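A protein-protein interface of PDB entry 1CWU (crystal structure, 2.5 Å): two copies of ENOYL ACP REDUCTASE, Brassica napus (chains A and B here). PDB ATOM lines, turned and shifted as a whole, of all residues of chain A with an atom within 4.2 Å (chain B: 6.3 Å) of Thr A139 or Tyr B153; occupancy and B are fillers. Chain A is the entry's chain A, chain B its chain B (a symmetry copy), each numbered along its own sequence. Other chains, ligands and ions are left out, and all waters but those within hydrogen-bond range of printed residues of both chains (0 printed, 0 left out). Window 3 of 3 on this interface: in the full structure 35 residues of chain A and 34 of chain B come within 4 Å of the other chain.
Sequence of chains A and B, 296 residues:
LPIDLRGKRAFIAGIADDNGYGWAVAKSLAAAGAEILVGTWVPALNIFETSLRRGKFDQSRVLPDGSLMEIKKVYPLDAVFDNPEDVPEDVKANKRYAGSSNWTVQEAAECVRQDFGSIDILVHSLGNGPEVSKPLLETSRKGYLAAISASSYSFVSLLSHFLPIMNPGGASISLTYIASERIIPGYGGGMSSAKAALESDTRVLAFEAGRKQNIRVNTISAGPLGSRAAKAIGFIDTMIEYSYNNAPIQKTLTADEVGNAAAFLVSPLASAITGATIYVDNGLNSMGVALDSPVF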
ATOM      1  N   GLU A 131     -19.460   9.123   8.693  1.00  0.00           N
ATOM      2  CA  GLU A 131     -20.091   9.879   7.587  1.00  0.00           C
ATOM      3  C   GLU A 131     -19.394  11.218   7.268  1.00  0.00           C
ATOM      4  O   GLU A 131     -20.022  12.179   6.805  1.00  0.00           O
ATOM      5  CB  GLU A 131     -21.559  10.159   7.909  1.00  0.00           C
ATOM      6  CG  GLU A 131     -22.414   8.916   8.013  1.00  0.00           C
ATOM      7  CD  GLU A 131     -23.841   9.210   8.431  1.00  0.00           C
ATOM      8  OE1 GLU A 131     -24.513  10.001   7.741  1.00  0.00           O
ATOM      9  OE2 GLU A 131     -24.236   8.774   9.536  1.00  0.00           O
ATOM     10  N   LYS A 134     -20.238  13.073   4.231  1.00  0.00           N
ATOM     11  CA  LYS A 134     -21.552  13.640   4.015  1.00  0.00           C
ATOM     12  C   LYS A 134     -21.730  15.036   4.608  1.00  0.00           C
ATOM     13  O   LYS A 134     -21.167  15.363   5.647  1.00  0.00           O
ATOM     14  CB  LYS A 134     -22.610  12.705   4.555  1.00  0.00           C
ATOM     15  CG  LYS A 134     -22.810  11.454   3.690  1.00  0.00           C
ATOM     16  CD  LYS A 134     -23.825  10.548   4.365  1.00  0.00           C
ATOM     17  CE  LYS A 134     -24.125   9.278   3.598  1.00  0.00           C
ATOM     18  NZ  LYS A 134     -25.147   8.491   4.348  1.00  0.00           N
ATOM     19  N   PRO A 135     -22.544  15.845   3.946  1.00  0.00           N
ATOM     20  CA  PRO A 135     -22.882  17.170   4.423  1.00  0.00           C
ATOM     21  C   PRO A 135     -23.680  16.999   5.682  1.00  0.00           C
ATOM     22  O   PRO A 135     -24.324  15.982   5.884  1.00  0.00           O
ATOM     23  CB  PRO A 135     -23.840  17.654   3.357  1.00  0.00           C
ATOM     24  CG  PRO A 135     -23.293  17.053   2.111  1.00  0.00           C
ATOM     25  CD  PRO A 135     -22.651  15.752   2.487  1.00  0.00           C
ATOM     26  N   LEU A 136     -23.703  18.010   6.513  1.00  0.00           N
ATOM     27  CA  LEU A 136     -24.523  17.901   7.691  1.00  0.00           C
ATOM     28  C   LEU A 136     -25.948  17.484   7.278  1.00  0.00           C
ATOM     29  O   LEU A 136     -26.569  16.648   7.942  1.00  0.00           O
ATOM     30  CB  LEU A 136     -24.545  19.223   8.450  1.00  0.00           C
ATOM     31  CG  LEU A 136     -23.471  19.342   9.514  1.00  0.00           C
ATOM     32  CD1 LEU A 136     -23.625  20.664  10.251  1.00  0.00           C
ATOM     33  CD2 LEU A 136     -23.656  18.174  10.486  1.00  0.00           C
ATOM     34  N   LEU A 137     -26.451  18.056   6.180  1.00  0.00           N
ATOM     35  CA  LEU A 137     -27.812  17.755   5.697  1.00  0.00           C
ATOM     36  C   LEU A 137     -28.021  16.276   5.407  1.00  0.00           C
ATOM     37  O   LEU A 137     -29.045  15.718   5.749  1.00  0.00           O
ATOM     38  CB  LEU A 137     -28.151  18.557   4.444  1.00  0.00           C
ATOM     39  CG  LEU A 137     -28.379  20.063   4.583  1.00  0.00           C
ATOM     40  CD1 LEU A 137     -28.513  20.630   3.199  1.00  0.00           C
ATOM     41  CD2 LEU A 137     -29.610  20.376   5.414  1.00  0.00           C
ATOM     42  N   GLU A 138     -27.037  15.635   4.801  1.00  0.00           N
ATOM     43  CA  GLU A 138     -27.116  14.202   4.499  1.00  0.00           C
ATOM     44  C   GLU A 138     -26.524  13.267   5.579  1.00  0.00           C
ATOM     45  O   GLU A 138     -26.254  12.107   5.316  1.00  0.00           O
ATOM     46  CB  GLU A 138     -26.465  13.932   3.153  1.00  0.00           C
ATOM     47  CG  GLU A 138     -27.083  14.755   2.062  1.00  0.00           C
ATOM     48  CD  GLU A 138     -26.534  14.444   0.704  1.00  0.00           C
ATOM     49  OE1 GLU A 138     -26.571  13.261   0.306  1.00  0.00           O
ATOM     50  OE2 GLU A 138     -26.006  15.377   0.058  1.00  0.00           O
ATOM     51  N   THR A 139     -26.297  13.801   6.772  1.00  0.00           N
ATOM     52  CA  THR A 139     -25.673  13.079   7.882  1.00  0.00           C
ATOM     53  C   THR A 139     -26.697  12.553   8.910  1.00  0.00           C
ATOM     54  O   THR A 139     -27.436  13.323   9.515  1.00  0.00           O
ATOM     55  CB  THR A 139     -24.636  14.029   8.611  1.00  0.00           C
ATOM     56  OG1 THR A 139     -23.547  14.339   7.734  1.00  0.00           O
ATOM     57  CG2 THR A 139     -24.111  13.442   9.922  1.00  0.00           C
ATOM     58  N   SER A 140     -26.674  11.248   9.152  1.00  0.00           N
ATOM     59  CA  SER A 140     -27.592  10.601  10.104  1.00  0.00           C
ATOM     60  C   SER A 140     -27.281  10.871  11.540  1.00  0.00           C
ATOM     61  O   SER A 140     -26.125  11.074  11.914  1.00  0.00           O
ATOM     62  CB  SER A 140     -27.581   9.082   9.911  1.00  0.00           C
ATOM     63  OG  SER A 140     -26.314   8.561  10.245  1.00  0.00           O
ATOM     64  N   ARG A 141     -28.304  10.774  12.370  1.00  0.00           N
ATOM     65  CA  ARG A 141     -28.119  10.978  13.793  1.00  0.00           C
ATOM     66  C   ARG A 141     -26.966  10.103  14.324  1.00  0.00           C
ATOM     67  O   ARG A 141     -26.086  10.572  15.063  1.00  0.00           O
ATOM     68  CB  ARG A 141     -29.403  10.621  14.552  1.00  0.00           C
ATOM     69  CG  ARG A 141     -29.259  10.827  16.076  1.00  0.00           C
ATOM     70  CD  ARG A 141     -30.594  10.830  16.796  1.00  0.00           C
ATOM     71  NE  ARG A 141     -31.594  11.681  16.154  1.00  0.00           N
ATOM     72  CZ  ARG A 141     -31.938  12.880  16.611  1.00  0.00           C
ATOM     73  NH1 ARG A 141     -31.362  13.361  17.711  1.00  0.00           N
ATOM     74  NH2 ARG A 141     -32.868  13.587  15.988  1.00  0.00           N
ATOM     75  N   TYR A 144     -23.558  11.230  13.158  1.00  0.00           N
ATOM     76  CA  TYR A 144     -23.245  12.465  13.852  1.00  0.00           C
ATOM     77  C   TYR A 144     -22.796  12.146  15.272  1.00  0.00           C
ATOM     78  O   TYR A 144     -21.747  12.598  15.761  1.00  0.00           O
ATOM     79  CB  TYR A 144     -24.506  13.339  13.869  1.00  0.00           C
ATOM     80  CG  TYR A 144     -24.342  14.743  14.441  1.00  0.00           C
ATOM     81  CD1 TYR A 144     -24.533  14.979  15.788  1.00  0.00           C
ATOM     82  CD2 TYR A 144     -24.152  15.837  13.602  1.00  0.00           C
ATOM     83  CE1 TYR A 144     -24.514  16.254  16.301  1.00  0.00           C
ATOM     84  CE2 TYR A 144     -24.104  17.122  14.110  1.00  0.00           C
ATOM     85  CZ  TYR A 144     -24.288  17.319  15.469  1.00  0.00           C
ATOM     86  OH  TYR A 144     -24.272  18.590  15.993  1.00  0.00           O
ATOM     87  N   GLY A 189     -20.116  14.950   8.168  1.00  0.00           N
ATOM     88  CA  GLY A 189     -20.512  13.917   9.098  1.00  0.00           C
ATOM     89  C   GLY A 189     -20.585  14.308  10.551  1.00  0.00           C
ATOM     90  O   GLY A 189     -20.706  13.437  11.411  1.00  0.00           O
ATOM     91  N   ALA B  79     -37.939  15.238  18.893  1.00  0.00           N
ATOM     92  CA  ALA B  79     -36.786  15.504  18.070  1.00  0.00           C
ATOM     93  C   ALA B  79     -35.578  14.548  18.223  1.00  0.00           C
ATOM     94  O   ALA B  79     -34.669  14.559  17.391  1.00  0.00           O
ATOM     95  CB  ALA B  79     -36.399  16.960  18.159  1.00  0.00           C
ATOM     96  N   VAL B  80     -35.574  13.685  19.236  1.00  0.00           N
ATOM     97  CA  VAL B  80     -34.503  12.714  19.309  1.00  0.00           C
ATOM     98  C   VAL B  80     -34.730  11.651  18.242  1.00  0.00           C
ATOM     99  O   VAL B  80     -33.789  10.968  17.845  1.00  0.00           O
ATOM    100  CB  VAL B  80     -34.435  11.993  20.638  1.00  0.00           C
ATOM    101  CG1 VAL B  80     -33.539  10.816  20.501  1.00  0.00           C
ATOM    102  CG2 VAL B  80     -33.901  12.890  21.704  1.00  0.00           C
ATOM    103  N   ASP B  82     -35.990  10.572  14.429  1.00  0.00           N
ATOM    104  CA  ASP B  82     -36.129  11.101  13.076  1.00  0.00           C
ATOM    105  C   ASP B  82     -37.102  10.357  12.190  1.00  0.00           C
ATOM    106  O   ASP B  82     -37.600  10.901  11.213  1.00  0.00           O
ATOM    107  CB  ASP B  82     -34.751  11.193  12.400  1.00  0.00           C
ATOM    108  CG  ASP B  82     -33.710  11.872  13.285  1.00  0.00           C
ATOM    109  OD1 ASP B  82     -34.069  12.854  13.979  1.00  0.00           O
ATOM    110  OD2 ASP B  82     -32.586  11.341  13.391  1.00  0.00           O
ATOM    111  N   HIS B 124     -36.449  26.404  16.186  1.00  0.00           N
ATOM    112  CA  HIS B 124     -36.004  25.306  17.060  1.00  0.00           C
ATOM    113  C   HIS B 124     -35.843  25.971  18.434  1.00  0.00           C
ATOM    114  O   HIS B 124     -35.147  26.984  18.574  1.00  0.00           O
ATOM    115  CB  HIS B 124     -34.650  24.751  16.531  1.00  0.00           C
ATOM    116  CG  HIS B 124     -33.995  23.719  17.409  1.00  0.00           C
ATOM    117  ND1 HIS B 124     -33.307  24.052  18.560  1.00  0.00           N
ATOM    118  CD2 HIS B 124     -33.770  22.401  17.209  1.00  0.00           C
ATOM    119  CE1 HIS B 124     -32.794  22.963  19.093  1.00  0.00           C
ATOM    120  NE2 HIS B 124     -33.039  21.952  18.281  1.00  0.00           N
ATOM    121  N   ALA B 147     -27.535  14.676  25.502  1.00  0.00           N
ATOM    122  CA  ALA B 147     -27.527  16.135  25.464  1.00  0.00           C
ATOM    123  C   ALA B 147     -27.266  16.665  24.061  1.00  0.00           C
ATOM    124  O   ALA B 147     -27.885  17.633  23.621  1.00  0.00           O
ATOM    125  CB  ALA B 147     -26.472  16.693  26.425  1.00  0.00           C
ATOM    126  N   ILE B 148     -26.330  16.051  23.364  1.00  0.00           N
ATOM    127  CA  ILE B 148     -25.969  16.530  22.038  1.00  0.00           C
ATOM    128  C   ILE B 148     -27.027  16.128  21.032  1.00  0.00           C
ATOM    129  O   ILE B 148     -27.238  16.804  20.017  1.00  0.00           O
ATOM    130  CB  ILE B 148     -24.590  15.955  21.611  1.00  0.00           C
ATOM    131  CG1 ILE B 148     -23.518  16.319  22.640  1.00  0.00           C
ATOM    132  CG2 ILE B 148     -24.128  16.581  20.304  1.00  0.00           C
ATOM    133  CD1 ILE B 148     -22.617  17.401  22.152  1.00  0.00           C
ATOM    134  N   SER B 149     -27.690  15.012  21.315  1.00  0.00           N
ATOM    135  CA  SER B 149     -28.711  14.468  20.418  1.00  0.00           C
ATOM    136  C   SER B 149     -30.013  15.249  20.433  1.00  0.00           C
ATOM    137  O   SER B 149     -30.607  15.507  19.383  1.00  0.00           O
ATOM    138  CB  SER B 149     -28.995  13.000  20.763  1.00  0.00           C
ATOM    139  OG  SER B 149     -30.055  12.493  19.969  1.00  0.00           O
ATOM    140  N   ALA B 150     -30.471  15.573  21.638  1.00  0.00           N
ATOM    141  CA  ALA B 150     -31.720  16.296  21.832  1.00  0.00           C
ATOM    142  C   ALA B 150     -31.511  17.785  21.557  1.00  0.00           C
ATOM    143  O   ALA B 150     -32.391  18.473  21.029  1.00  0.00           O
ATOM    144  CB  ALA B 150     -32.239  16.093  23.282  1.00  0.00           C
ATOM    145  N   SER B 151     -30.346  18.282  21.957  1.00  0.00           N
ATOM    146  CA  SER B 151     -30.028  19.680  21.799  1.00  0.00           C
ATOM    147  C   SER B 151     -29.370  20.155  20.488  1.00  0.00           C
ATOM    148  O   SER B 151     -29.667  21.246  20.026  1.00  0.00           O
ATOM    149  CB  SER B 151     -29.271  20.170  23.010  1.00  0.00           C
ATOM    150  OG  SER B 151     -29.988  19.870  24.204  1.00  0.00           O
ATOM    151  N   SER B 152     -28.433  19.393  19.926  1.00  0.00           N
ATOM    152  CA  SER B 152     -27.768  19.816  18.677  1.00  0.00           C
ATOM    153  C   SER B 152     -28.328  19.111  17.447  1.00  0.00           C
ATOM    154  O   SER B 152     -28.896  19.757  16.565  1.00  0.00           O
ATOM    155  CB  SER B 152     -26.233  19.637  18.722  1.00  0.00           C
ATOM    156  OG  SER B 152     -25.650  20.312  19.817  1.00  0.00           O
ATOM    157  N   TYR B 153     -28.172  17.786  17.389  1.00  0.00           N
ATOM    158  CA  TYR B 153     -28.639  17.045  16.232  1.00  0.00           C
ATOM    159  C   TYR B 153     -30.124  17.257  15.889  1.00  0.00           C
ATOM    160  O   TYR B 153     -30.487  17.328  14.713  1.00  0.00           O
ATOM    161  CB  TYR B 153     -28.271  15.562  16.289  1.00  0.00           C
ATOM    162  CG  TYR B 153     -28.504  14.896  14.969  1.00  0.00           C
ATOM    163  CD1 TYR B 153     -27.532  14.924  13.986  1.00  0.00           C
ATOM    164  CD2 TYR B 153     -29.764  14.415  14.634  1.00  0.00           C
ATOM    165  CE1 TYR B 153     -27.787  14.444  12.729  1.00  0.00           C
ATOM    166  CE2 TYR B 153     -29.996  13.826  13.403  1.00  0.00           C
ATOM    167  CZ  TYR B 153     -29.005  13.852  12.459  1.00  0.00           C
ATOM    168  OH  TYR B 153     -29.258  13.362  11.223  1.00  0.00           O
ATOM    169  N   SER B 154     -30.981  17.409  16.894  1.00  0.00           N
ATOM    170  CA  SER B 154     -32.379  17.682  16.582  1.00  0.00           C
ATOM    171  C   SER B 154     -32.507  18.865  15.596  1.00  0.00           C
ATOM    172  O   SER B 154     -33.333  18.841  14.664  1.00  0.00           O
ATOM    173  CB  SER B 154     -33.193  17.932  17.847  1.00  0.00           C
ATOM    174  OG  SER B 154     -32.749  19.083  18.527  1.00  0.00           O
ATOM    175  N   PHE B 155     -31.665  19.880  15.734  1.00  0.00           N
ATOM    176  CA  PHE B 155     -31.802  20.966  14.783  1.00  0.00           C
ATOM    177  C   PHE B 155     -31.470  20.491  13.412  1.00  0.00           C
ATOM    178  O   PHE B 155     -32.144  20.808  12.424  1.00  0.00           O
ATOM    179  CB  PHE B 155     -30.954  22.195  15.099  1.00  0.00           C
ATOM    180  CG  PHE B 155     -30.990  23.219  13.987  1.00  0.00           C
ATOM    181  CD1 PHE B 155     -32.072  24.091  13.860  1.00  0.00           C
ATOM    182  CD2 PHE B 155     -30.005  23.229  13.000  1.00  0.00           C
ATOM    183  CE1 PHE B 155     -32.140  24.980  12.806  1.00  0.00           C
ATOM    184  CE2 PHE B 155     -30.072  24.102  11.919  1.00  0.00           C
ATOM    185  CZ  PHE B 155     -31.137  24.982  11.823  1.00  0.00           C
ATOM    186  N   VAL B 156     -30.392  19.737  13.336  1.00  0.00           N
ATOM    187  CA  VAL B 156     -29.972  19.244  12.054  1.00  0.00           C
ATOM    188  C   VAL B 156     -31.105  18.479  11.413  1.00  0.00           C
ATOM    189  O   VAL B 156     -31.420  18.680  10.250  1.00  0.00           O
ATOM    190  CB  VAL B 156     -28.747  18.328  12.176  1.00  0.00           C
ATOM    191  CG1 VAL B 156     -28.389  17.766  10.792  1.00  0.00           C
ATOM    192  CG2 VAL B 156     -27.542  19.109  12.776  1.00  0.00           C
ATOM    193  N   SER B 157     -31.723  17.603  12.196  1.00  0.00           N
ATOM    194  CA  SER B 157     -32.796  16.753  11.718  1.00  0.00           C
ATOM    195  C   SER B 157     -33.989  17.563  11.270  1.00  0.00           C
ATOM    196  O   SER B 157     -34.493  17.374  10.167  1.00  0.00           O
ATOM    197  CB  SER B 157     -33.209  15.755  12.801  1.00  0.00           C
ATOM    198  OG  SER B 157     -34.480  15.209  12.506  1.00  0.00           O
ATOM    199  N   LEU B 158     -34.444  18.470  12.125  1.00  0.00           N
ATOM    200  CA  LEU B 158     -35.586  19.281  11.759  1.00  0.00           C
ATOM    201  C   LEU B 158     -35.335  19.986  10.447  1.00  0.00           C
ATOM    202  O   LEU B 158     -36.063  19.791   9.454  1.00  0.00           O
ATOM    203  CB  LEU B 158     -35.887  20.286  12.855  1.00  0.00           C
ATOM    204  CG  LEU B 158     -36.822  19.645  13.868  1.00  0.00           C
ATOM    205  CD1 LEU B 158     -36.846  20.395  15.155  1.00  0.00           C
ATOM    206  CD2 LEU B 158     -38.234  19.523  13.260  1.00  0.00           C
ATOM    207  N   SER B 160     -33.088  19.524   8.148  1.00  0.00           N
ATOM    208  CA  SER B 160     -32.886  18.607   7.051  1.00  0.00           C
ATOM    209  C   SER B 160     -34.186  18.066   6.579  1.00  0.00           C
ATOM    210  O   SER B 160     -34.390  17.939   5.356  1.00  0.00           O
ATOM    211  CB  SER B 160     -32.004  17.455   7.494  1.00  0.00           C
ATOM    212  OG  SER B 160     -31.573  16.701   6.381  1.00  0.00           O
ATOM    213  N   HIS B 161     -35.088  17.791   7.495  1.00  0.00           N
ATOM    214  CA  HIS B 161     -36.342  17.245   7.080  1.00  0.00           C
ATOM    215  C   HIS B 161     -37.310  18.239   6.410  1.00  0.00           C
ATOM    216  O   HIS B 161     -37.857  17.997   5.333  1.00  0.00           O
ATOM    217  CB  HIS B 161     -36.996  16.520   8.253  1.00  0.00           C
ATOM    218  CG  HIS B 161     -36.429  15.147   8.488  1.00  0.00           C
ATOM    219  ND1 HIS B 161     -35.575  14.867   9.539  1.00  0.00           N
ATOM    220  CD2 HIS B 161     -36.596  13.983   7.820  1.00  0.00           C
ATOM    221  CE1 HIS B 161     -35.234  13.590   9.494  1.00  0.00           C
ATOM    222  NE2 HIS B 161     -35.839  13.029   8.469  1.00  0.00           N
ATOM    223  N   ASP B 201     -23.026  24.198  13.741  1.00  0.00           N
ATOM    224  CA  ASP B 201     -23.895  23.757  12.637  1.00  0.00           C
ATOM    225  C   ASP B 201     -24.725  24.858  12.001  1.00  0.00           C
ATOM    226  O   ASP B 201     -25.172  24.710  10.859  1.00  0.00           O
ATOM    227  CB  ASP B 201     -24.814  22.618  13.059  1.00  0.00           C
ATOM    228  CG  ASP B 201     -24.064  21.406  13.531  1.00  0.00           C
ATOM    229  OD1 ASP B 201     -22.963  21.126  12.994  1.00  0.00           O
ATOM    230  OD2 ASP B 201     -24.640  20.692  14.380  1.00  0.00           O
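Of the 11 printed residues of chain A, 6 touch a printed residue of chain B. Printed residues of chain A that touch a printed residue of chain B: Leu A136, Leu A137, Thr A139, Ser A140, Arg A141 and Tyr A144. Hydrophobic or aromatic side chains of chain A that line the printed part of chain B: Leu A136 and Tyr A144. Hydrophobic or aromatic side chains of chain B within 4 Å of the printed part of chain A: Tyr B153 and Val B156. Among the printed residues, 14 pairs touch across the chains. Among the printed residues, Asp or Glu carboxylates within 4 Å of a Lys or Arg side-chain nitrogen of the other chain: Arg A141 with Asp B82 (2.5 Å).
Of the printed residues of chain B, Thr A139 touches Tyr B153 (2.5 Å). Tyr B153 touches just these residues of chain A: Thr A139, Ser A140, Arg A141 and Tyr A144. Printed residues of chain A within 4 Å of Ser B160: Leu A137. Of the printed residues of chain A, Ser B157 touches Arg A141 (3.9 Å). Of the printed residues of chain B, Leu A136 touches Val B156 (3.6 Å) and Asp B201 (2.9 Å). Printed residues of chain B within 4 Å of Leu A137: Ser B160. Of the printed residues of chain A, Val B80 touches Arg A141. The nearest residue of chain B that does not touch Thr A139 is Val B156 (4.7 Å). The nearest printed residue of chain A that does not touch Tyr B153 is Leu A136 (5.4 Å).
N of Ser A140 lies within hydrogen-bond range of OE1 of Glu A131 (2.9 Å). The side-chain carboxylate of Asp B82 lies within hydrogen-bond range of the side-chain hydroxyl of Ser B157. The backbone carbonyl oxygen (O) of Ile B148 lies within hydrogen-bond range of the backbone NH (N) of Tyr B153, 3.0 Å away. The side-chain hydroxyl of Thr A139 lies within hydrogen-bond range of the backbone carbonyl oxygen of Pro A135 (2.6 Å). The backbone carbonyl oxygen (O) of Ser B149 sits at hydrogen-bond distance from the backbone NH (N) of Ser B154. The backbone carbonyl oxygen of Lys A134 sits at hydrogen-bond distance from the side-chain hydroxyl of Thr A139.
No position is printed for both chains.
Among the printed residues, pairs that only touch across the chains: Leu A136 with Asp B201 (2.9 Å), Ser A140 with Tyr B153 (3.2 Å), Tyr A144 with Tyr B153 (3.2 Å), Tyr A144 with Ser B152 (3.5 Å), Leu A136 with Val B156 (3.6 Å) and Arg A141 with Ser B157 (3.9 Å).
OG of Ser B160 lies within hydrogen-bond range of O of Leu A137 (2.8 Å). NH2 of Arg A141 lies within salt-bridge range of OD1 of Asp B82, 2.5 Å away. The backbone carbonyl oxygen (O) of Ala B79 is in hydrogen-bond range of the guanidinium group (NH2) of Arg A141, 2.5 Å away. NH1 of Arg A141 is in hydrogen-bond range of OG of Ser B149, 2.7 Å away. The side-chain hydroxyl of Tyr A144 is in hydrogen-bond range of the side-chain carboxylate of Asp B201 (2.7 Å). The backbone NH of Arg A141 sits at hydrogen-bond distance from the side-chain hydroxyl of Tyr B153 (3.0 Å). The backbone carbonyl oxygen of Thr A139 sits at hydrogen-bond distance from the side-chain hydroxyl of Tyr B153, 2.5 Å away. O of Val B80 is in hydrogen-bond range of NE of Arg A141 (2.9 Å).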
